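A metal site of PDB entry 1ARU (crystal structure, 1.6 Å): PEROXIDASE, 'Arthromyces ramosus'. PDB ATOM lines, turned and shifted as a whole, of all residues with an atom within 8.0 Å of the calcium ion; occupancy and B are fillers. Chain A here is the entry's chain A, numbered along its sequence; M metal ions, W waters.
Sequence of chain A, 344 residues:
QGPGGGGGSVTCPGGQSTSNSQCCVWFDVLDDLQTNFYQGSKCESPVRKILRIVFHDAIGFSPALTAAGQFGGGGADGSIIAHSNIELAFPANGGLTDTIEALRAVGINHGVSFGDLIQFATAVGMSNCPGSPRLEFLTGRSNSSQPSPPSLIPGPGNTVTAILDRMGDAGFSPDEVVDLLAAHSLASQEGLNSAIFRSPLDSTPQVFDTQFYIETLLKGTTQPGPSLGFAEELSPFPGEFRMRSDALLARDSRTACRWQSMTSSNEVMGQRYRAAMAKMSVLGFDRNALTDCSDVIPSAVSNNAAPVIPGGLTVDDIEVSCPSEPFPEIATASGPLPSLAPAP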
ATOM      1  N   ILE A  53      12.845   6.118 -25.942  1.00  0.00           N
ATOM      2  CA  ILE A  53      13.976   6.991 -25.632  1.00  0.00           C
ATOM      3  C   ILE A  53      15.081   6.930 -26.684  1.00  0.00           C
ATOM      4  O   ILE A  53      15.578   7.980 -27.098  1.00  0.00           O
ATOM      5  CB  ILE A  53      14.521   6.615 -24.212  1.00  0.00           C
ATOM      6  CG1 ILE A  53      13.527   7.129 -23.163  1.00  0.00           C
ATOM      7  CG2 ILE A  53      15.849   7.289 -23.926  1.00  0.00           C
ATOM      8  CD1 ILE A  53      13.778   6.523 -21.773  1.00  0.00           C
ATOM      9  N   VAL A  54      15.484   5.779 -27.212  1.00  0.00           N
ATOM     10  CA  VAL A  54      16.580   5.742 -28.158  1.00  0.00           C
ATOM     11  C   VAL A  54      16.189   6.443 -29.461  1.00  0.00           C
ATOM     12  O   VAL A  54      17.017   7.173 -30.001  1.00  0.00           O
ATOM     13  CB  VAL A  54      17.012   4.248 -28.359  1.00  0.00           C
ATOM     14  CG1 VAL A  54      16.019   3.434 -29.137  1.00  0.00           C
ATOM     15  CG2 VAL A  54      18.354   4.256 -29.045  1.00  0.00           C
ATOM     16  N   PHE A  55      14.924   6.304 -29.888  1.00  0.00           N
ATOM     17  CA  PHE A  55      14.393   6.972 -31.076  1.00  0.00           C
ATOM     18  C   PHE A  55      14.371   8.485 -30.804  1.00  0.00           C
ATOM     19  O   PHE A  55      14.951   9.257 -31.583  1.00  0.00           O
ATOM     20  CB  PHE A  55      12.957   6.458 -31.363  1.00  0.00           C
ATOM     21  CG  PHE A  55      12.212   7.155 -32.498  1.00  0.00           C
ATOM     22  CD1 PHE A  55      12.876   7.596 -33.638  1.00  0.00           C
ATOM     23  CD2 PHE A  55      10.846   7.359 -32.398  1.00  0.00           C
ATOM     24  CE1 PHE A  55      12.179   8.233 -34.655  1.00  0.00           C
ATOM     25  CE2 PHE A  55      10.142   7.982 -33.409  1.00  0.00           C
ATOM     26  CZ  PHE A  55      10.810   8.425 -34.536  1.00  0.00           C
ATOM     27  N   HIS A  56      13.789   8.920 -29.695  1.00  0.00           N
ATOM     28  CA  HIS A  56      13.696  10.358 -29.426  1.00  0.00           C
ATOM     29  C   HIS A  56      15.029  11.022 -29.171  1.00  0.00           C
ATOM     30  O   HIS A  56      15.176  12.223 -29.398  1.00  0.00           O
ATOM     31  CB  HIS A  56      12.757  10.597 -28.237  1.00  0.00           C
ATOM     32  CG  HIS A  56      11.301  10.249 -28.545  1.00  0.00           C
ATOM     33  ND1 HIS A  56      10.253  10.560 -27.787  1.00  0.00           N
ATOM     34  CD2 HIS A  56      10.823   9.503 -29.605  1.00  0.00           C
ATOM     35  CE1 HIS A  56       9.185  10.030 -28.335  1.00  0.00           C
ATOM     36  NE2 HIS A  56       9.536   9.395 -29.436  1.00  0.00           N
ATOM     37  N   ASP A  57      15.995  10.267 -28.711  1.00  0.00           N
ATOM     38  CA  ASP A  57      17.321  10.813 -28.558  1.00  0.00           C
ATOM     39  C   ASP A  57      18.007  10.935 -29.931  1.00  0.00           C
ATOM     40  O   ASP A  57      18.473  12.029 -30.265  1.00  0.00           O
ATOM     41  CB  ASP A  57      18.225   9.945 -27.640  1.00  0.00           C
ATOM     42  CG  ASP A  57      19.602  10.561 -27.407  1.00  0.00           C
ATOM     43  OD1 ASP A  57      19.716  11.794 -27.373  1.00  0.00           O
ATOM     44  OD2 ASP A  57      20.550   9.803 -27.287  1.00  0.00           O
ATOM     45  N   ALA A  58      18.000   9.874 -30.731  1.00  0.00           N
ATOM     46  CA  ALA A  58      18.738   9.893 -31.977  1.00  0.00           C
ATOM     47  C   ALA A  58      18.130  10.752 -33.053  1.00  0.00           C
ATOM     48  O   ALA A  58      18.879  11.404 -33.793  1.00  0.00           O
ATOM     49  CB  ALA A  58      18.893   8.470 -32.489  1.00  0.00           C
ATOM     50  N   ILE A  59      16.798  10.843 -33.103  1.00  0.00           N
ATOM     51  CA  ILE A  59      16.140  11.650 -34.119  1.00  0.00           C
ATOM     52  C   ILE A  59      16.313  13.167 -33.946  1.00  0.00           C
ATOM     53  O   ILE A  59      15.982  13.913 -34.887  1.00  0.00           O
ATOM     54  CB  ILE A  59      14.630  11.213 -34.178  1.00  0.00           C
ATOM     55  CG1 ILE A  59      14.139  11.438 -35.616  1.00  0.00           C
ATOM     56  CG2 ILE A  59      13.735  11.995 -33.233  1.00  0.00           C
ATOM     57  CD1 ILE A  59      14.851  10.572 -36.650  1.00  0.00           C
ATOM     58  N   GLY A  60      16.829  13.691 -32.821  1.00  0.00           N
ATOM     59  CA  GLY A  60      17.082  15.120 -32.714  1.00  0.00           C
ATOM     60  C   GLY A  60      18.378  15.398 -33.473  1.00  0.00           C
ATOM     61  O   GLY A  60      19.453  15.595 -32.885  1.00  0.00           O
ATOM     62  N   PHE A  61      18.284  15.376 -34.800  1.00  0.00           N
ATOM     63  CA  PHE A  61      19.419  15.566 -35.695  1.00  0.00           C
ATOM     64  C   PHE A  61      18.803  16.049 -37.010  1.00  0.00           C
ATOM     65  O   PHE A  61      18.005  15.349 -37.648  1.00  0.00           O
ATOM     66  CB  PHE A  61      20.125  14.239 -35.860  1.00  0.00           C
ATOM     67  CG  PHE A  61      21.308  14.262 -36.798  1.00  0.00           C
ATOM     68  CD1 PHE A  61      22.469  14.878 -36.420  1.00  0.00           C
ATOM     69  CD2 PHE A  61      21.192  13.634 -38.030  1.00  0.00           C
ATOM     70  CE1 PHE A  61      23.533  14.874 -37.299  1.00  0.00           C
ATOM     71  CE2 PHE A  61      22.278  13.651 -38.899  1.00  0.00           C
ATOM     72  CZ  PHE A  61      23.442  14.268 -38.530  1.00  0.00           C
ATOM     73  N   GLY A  73      21.117  19.665 -33.837  1.00  0.00           N
ATOM     74  CA  GLY A  73      20.958  18.538 -32.918  1.00  0.00           C
ATOM     75  C   GLY A  73      22.169  17.621 -33.019  1.00  0.00           C
ATOM     76  O   GLY A  73      22.783  17.542 -34.064  1.00  0.00           O
ATOM     77  N   GLY A  74      22.570  16.956 -31.944  1.00  0.00           N
ATOM     78  CA  GLY A  74      23.739  16.089 -32.001  1.00  0.00           C
ATOM     79  C   GLY A  74      23.386  14.620 -32.247  1.00  0.00           C
ATOM     80  O   GLY A  74      24.280  13.773 -32.125  1.00  0.00           O
ATOM     81  N   GLY A  75      22.136  14.265 -32.532  1.00  0.00           N
ATOM     82  CA  GLY A  75      21.816  12.875 -32.800  1.00  0.00           C
ATOM     83  C   GLY A  75      21.797  12.012 -31.551  1.00  0.00           C
ATOM     84  O   GLY A  75      21.260  12.442 -30.512  1.00  0.00           O
ATOM     85  N   ALA A  76      22.421  10.828 -31.623  1.00  0.00           N
ATOM     86  CA  ALA A  76      22.438   9.852 -30.557  1.00  0.00           C
ATOM     87  C   ALA A  76      23.480  10.199 -29.502  1.00  0.00           C
ATOM     88  O   ALA A  76      24.338   9.393 -29.121  1.00  0.00           O
ATOM     89  CB  ALA A  76      22.739   8.477 -31.159  1.00  0.00           C
ATOM     90  N   ASP A  77      23.327  11.397 -28.918  1.00  0.00           N
ATOM     91  CA  ASP A  77      24.259  11.965 -27.955  1.00  0.00           C
ATOM     92  C   ASP A  77      23.872  11.915 -26.473  1.00  0.00           C
ATOM     93  O   ASP A  77      24.556  12.478 -25.615  1.00  0.00           O
ATOM     94  CB  ASP A  77      24.516  13.424 -28.358  1.00  0.00           C
ATOM     95  CG  ASP A  77      23.262  14.303 -28.418  1.00  0.00           C
ATOM     96  OD1 ASP A  77      22.162  13.837 -28.080  1.00  0.00           O
ATOM     97  OD2 ASP A  77      23.399  15.459 -28.794  1.00  0.00           O
ATOM     98  N   GLY A  78      22.745  11.306 -26.139  1.00  0.00           N
ATOM     99  CA  GLY A  78      22.289  11.265 -24.757  1.00  0.00           C
ATOM    100  C   GLY A  78      21.740  12.602 -24.253  1.00  0.00           C
ATOM    101  O   GLY A  78      21.518  12.775 -23.038  1.00  0.00           O
ATOM    102  N   SER A  79      21.410  13.548 -25.161  1.00  0.00           N
ATOM    103  CA  SER A  79      20.937  14.859 -24.750  1.00  0.00           C
ATOM    104  C   SER A  79      19.569  14.740 -24.106  1.00  0.00           C
ATOM    105  O   SER A  79      19.234  15.628 -23.315  1.00  0.00           O
ATOM    106  CB  SER A  79      20.846  15.797 -25.934  1.00  0.00           C
ATOM    107  OG  SER A  79      19.910  15.303 -26.912  1.00  0.00           O
ATOM    108  N   ILE A  80      18.750  13.699 -24.383  1.00  0.00           N
ATOM    109  CA  ILE A  80      17.467  13.587 -23.696  1.00  0.00           C
ATOM    110  C   ILE A  80      17.645  13.381 -22.181  1.00  0.00           C
ATOM    111  O   ILE A  80      16.759  13.722 -21.390  1.00  0.00           O
ATOM    112  CB  ILE A  80      16.654  12.438 -24.423  1.00  0.00           C
ATOM    113  CG1 ILE A  80      15.166  12.453 -23.971  1.00  0.00           C
ATOM    114  CG2 ILE A  80      17.341  11.090 -24.189  1.00  0.00           C
ATOM    115  CD1 ILE A  80      14.190  11.599 -24.801  1.00  0.00           C
ATOM    116  N   ILE A  81      18.800  12.861 -21.752  1.00  0.00           N
ATOM    117  CA  ILE A  81      19.094  12.691 -20.328  1.00  0.00           C
ATOM    118  C   ILE A  81      19.828  13.946 -19.833  1.00  0.00           C
ATOM    119  O   ILE A  81      19.346  14.622 -18.939  1.00  0.00           O
ATOM    120  CB  ILE A  81      19.981  11.433 -20.051  1.00  0.00           C
ATOM    121  CG1 ILE A  81      19.269  10.167 -20.528  1.00  0.00           C
ATOM    122  CG2 ILE A  81      20.303  11.357 -18.542  1.00  0.00           C
ATOM    123  CD1 ILE A  81      20.001   8.863 -20.229  1.00  0.00           C
ATOM    124  N   HIS A  83      19.958  16.877 -20.944  1.00  0.00           N
ATOM    125  CA  HIS A  83      19.133  18.074 -21.022  1.00  0.00           C
ATOM    126  C   HIS A  83      17.676  17.703 -20.892  1.00  0.00           C
ATOM    127  O   HIS A  83      16.832  18.259 -21.587  1.00  0.00           O
ATOM    128  CB  HIS A  83      19.355  18.792 -22.339  1.00  0.00           C
ATOM    129  CG  HIS A  83      20.809  19.196 -22.445  1.00  0.00           C
ATOM    130  ND1 HIS A  83      21.417  20.221 -21.712  1.00  0.00           N
ATOM    131  CD2 HIS A  83      21.730  18.552 -23.267  1.00  0.00           C
ATOM    132  CE1 HIS A  83      22.707  20.220 -22.130  1.00  0.00           C
ATOM    133  NE2 HIS A  83      22.905  19.278 -23.011  1.00  0.00           N
ATOM    134  N   GLU A  87      14.249  18.872 -22.919  1.00  0.00           N
ATOM    135  CA  GLU A  87      13.662  17.943 -23.858  1.00  0.00           C
ATOM    136  C   GLU A  87      12.412  17.233 -23.378  1.00  0.00           C
ATOM    137  O   GLU A  87      11.550  16.889 -24.193  1.00  0.00           O
ATOM    138  CB  GLU A  87      14.693  16.908 -24.297  1.00  0.00           C
ATOM    139  CG  GLU A  87      15.817  17.548 -25.069  1.00  0.00           C
ATOM    140  CD  GLU A  87      16.663  16.535 -25.844  1.00  0.00           C
ATOM    141  OE1 GLU A  87      16.167  15.466 -26.239  1.00  0.00           O
ATOM    142  OE2 GLU A  87      17.831  16.850 -26.067  1.00  0.00           O
ATOM    143  N   GLY A 115      24.940   8.873 -24.151  1.00  0.00           N
ATOM    144  CA  GLY A 115      24.605   8.427 -25.509  1.00  0.00           C
ATOM    145  C   GLY A 115      24.888   6.946 -25.679  1.00  0.00           C
ATOM    146  O   GLY A 115      24.075   6.190 -26.222  1.00  0.00           O
ATOM    147  N   ILE A 118      22.319   4.735 -23.567  1.00  0.00           N
ATOM    148  CA  ILE A 118      21.018   4.527 -24.166  1.00  0.00           C
ATOM    149  C   ILE A 118      21.090   3.454 -25.249  1.00  0.00           C
ATOM    150  O   ILE A 118      20.217   2.586 -25.311  1.00  0.00           O
ATOM    151  CB  ILE A 118      20.490   5.885 -24.726  1.00  0.00           C
ATOM    152  CG1 ILE A 118      20.072   6.788 -23.566  1.00  0.00           C
ATOM    153  CG2 ILE A 118      19.276   5.656 -25.617  1.00  0.00           C
ATOM    154  CD1 ILE A 118      19.789   8.262 -23.966  1.00  0.00           C
ATOM    155  N   SER A 145      26.851  17.171 -24.743  1.00  0.00           N
ATOM    156  CA  SER A 145      25.794  17.412 -25.704  1.00  0.00           C
ATOM    157  C   SER A 145      25.162  18.775 -25.475  1.00  0.00           C
ATOM    158  O   SER A 145      25.383  19.449 -24.456  1.00  0.00           O
ATOM    159  CB  SER A 145      24.735  16.320 -25.561  1.00  0.00           C
ATOM    160  OG  SER A 145      24.260  16.312 -24.225  1.00  0.00           O
ATOM    161  N   GLN A 146      24.412  19.216 -26.459  1.00  0.00           N
ATOM    162  CA  GLN A 146      23.628  20.449 -26.399  1.00  0.00           C
ATOM    163  C   GLN A 146      22.199  19.947 -26.521  1.00  0.00           C
ATOM    164  O   GLN A 146      21.992  18.834 -27.048  1.00  0.00           O
ATOM    165  CB  GLN A 146      23.915  21.324 -27.567  1.00  0.00           C
ATOM    166  CG  GLN A 146      25.099  22.207 -27.311  1.00  0.00           C
ATOM    167  CD  GLN A 146      25.670  22.541 -28.670  1.00  0.00           C
ATOM    168  OE1 GLN A 146      26.565  21.817 -29.124  1.00  0.00           O
ATOM    169  NE2 GLN A 146      25.160  23.548 -29.391  1.00  0.00           N
ATOM    170  N   PRO A 147      21.186  20.685 -26.055  1.00  0.00           N
ATOM    171  CA  PRO A 147      19.784  20.305 -26.153  1.00  0.00           C
ATOM    172  C   PRO A 147      19.325  20.118 -27.583  1.00  0.00           C
ATOM    173  O   PRO A 147      19.702  20.882 -28.482  1.00  0.00           O
ATOM    174  CB  PRO A 147      19.026  21.428 -25.483  1.00  0.00           C
ATOM    175  CG  PRO A 147      20.050  22.127 -24.653  1.00  0.00           C
ATOM    176  CD  PRO A 147      21.272  22.039 -25.535  1.00  0.00           C
ATOM    177  N   SER A 148      18.491  19.115 -27.839  1.00  0.00           N
ATOM    178  CA  SER A 148      17.921  18.907 -29.152  1.00  0.00           C
ATOM    179  C   SER A 148      17.025  20.117 -29.437  1.00  0.00           C
ATOM    180  O   SER A 148      16.387  20.682 -28.527  1.00  0.00           O
ATOM    181  CB  SER A 148      17.087  17.632 -29.170  1.00  0.00           C
ATOM    182  OG  SER A 148      16.372  17.497 -30.389  1.00  0.00           O
ATOM    183  N   PRO A 149      17.007  20.625 -30.686  1.00  0.00           N
ATOM    184  CA  PRO A 149      16.066  21.633 -31.118  1.00  0.00           C
ATOM    185  C   PRO A 149      14.674  21.019 -30.960  1.00  0.00           C
ATOM    186  O   PRO A 149      14.538  19.790 -30.947  1.00  0.00           O
ATOM    187  CB  PRO A 149      16.443  21.889 -32.548  1.00  0.00           C
ATOM    188  CG  PRO A 149      17.916  21.516 -32.606  1.00  0.00           C
ATOM    189  CD  PRO A 149      17.928  20.263 -31.756  1.00  0.00           C
ATOM    190  N   LEU A 283      23.746   8.417 -35.622  1.00  0.00           N
ATOM    191  CA  LEU A 283      23.356   9.717 -36.137  1.00  0.00           C
ATOM    192  C   LEU A 283      24.081  10.768 -35.293  1.00  0.00           C
ATOM    193  O   LEU A 283      23.981  10.765 -34.063  1.00  0.00           O
ATOM    194  CB  LEU A 283      21.826   9.860 -36.030  1.00  0.00           C
ATOM    195  CG  LEU A 283      20.871   9.838 -37.251  1.00  0.00           C
ATOM    196  CD1 LEU A 283      21.265   8.851 -38.322  1.00  0.00           C
ATOM    197  CD2 LEU A 283      19.498   9.570 -36.681  1.00  0.00           C
ATOM    198  N   PHE A 285      27.445  11.023 -35.449  1.00  0.00           N
ATOM    199  CA  PHE A 285      28.766  10.458 -35.166  1.00  0.00           C
ATOM    200  C   PHE A 285      29.334   9.748 -36.388  1.00  0.00           C
ATOM    201  O   PHE A 285      28.629   9.443 -37.365  1.00  0.00           O
ATOM    202  CB  PHE A 285      28.717   9.402 -34.027  1.00  0.00           C
ATOM    203  CG  PHE A 285      28.303  10.020 -32.705  1.00  0.00           C
ATOM    204  CD1 PHE A 285      26.955  10.186 -32.441  1.00  0.00           C
ATOM    205  CD2 PHE A 285      29.261  10.486 -31.829  1.00  0.00           C
ATOM    206  CE1 PHE A 285      26.555  10.846 -31.280  1.00  0.00           C
ATOM    207  CE2 PHE A 285      28.864  11.147 -30.678  1.00  0.00           C
ATOM    208  CZ  PHE A 285      27.509  11.320 -30.405  1.00  0.00           C
HETATM  209 CA    CA M   1      19.828  13.619 -28.768  1.00  0.00          CA
HETATM  210  O   HOH W   1      17.399  14.132 -28.258  1.00  0.00           O
HETATM  211  O   HOH W   2      19.727  15.531 -30.286  1.00  0.00           O
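Water W1 lies within hydrogen-bond range of OE1 of Glu 87 (2.7 Å) and O of His 56 (3.1 Å).
The calcium ion is bound by the side-chain carboxylate (OD1) of Asp 57 (2.3 Å), water W2 (2.4 Å), the side-chain carboxylate (OD1) of Asp 77 (2.4 Å), the side-chain hydroxyl (OG) of Ser 79 (2.5 Å), water W1 (2.5 Å), the backbone carbonyl oxygen (O) of Gly 75 (2.5 Å) and the backbone carbonyl oxygen (O) of Asp 57 (2.6 Å).
Four residues have an atom within 4 Å of the calcium ion: Asp 57, Gly 75, Asp 77 and Ser 79. The nearest printed residue that does not touch the calcium ion is Ile 80 (4.5 Å).
N of Gly 78 is in hydrogen-bond range of OD2 of Asp 57 (2.9 Å). The side-chain hydroxyl (OG) of Ser 79 lies close to the side-chain carboxylate (OE2) of Glu 87 (2.7 Å). The backbone NH (N) of Gly 75 lies within hydrogen-bond range of the backbone carbonyl oxygen (O) of Gly 60.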
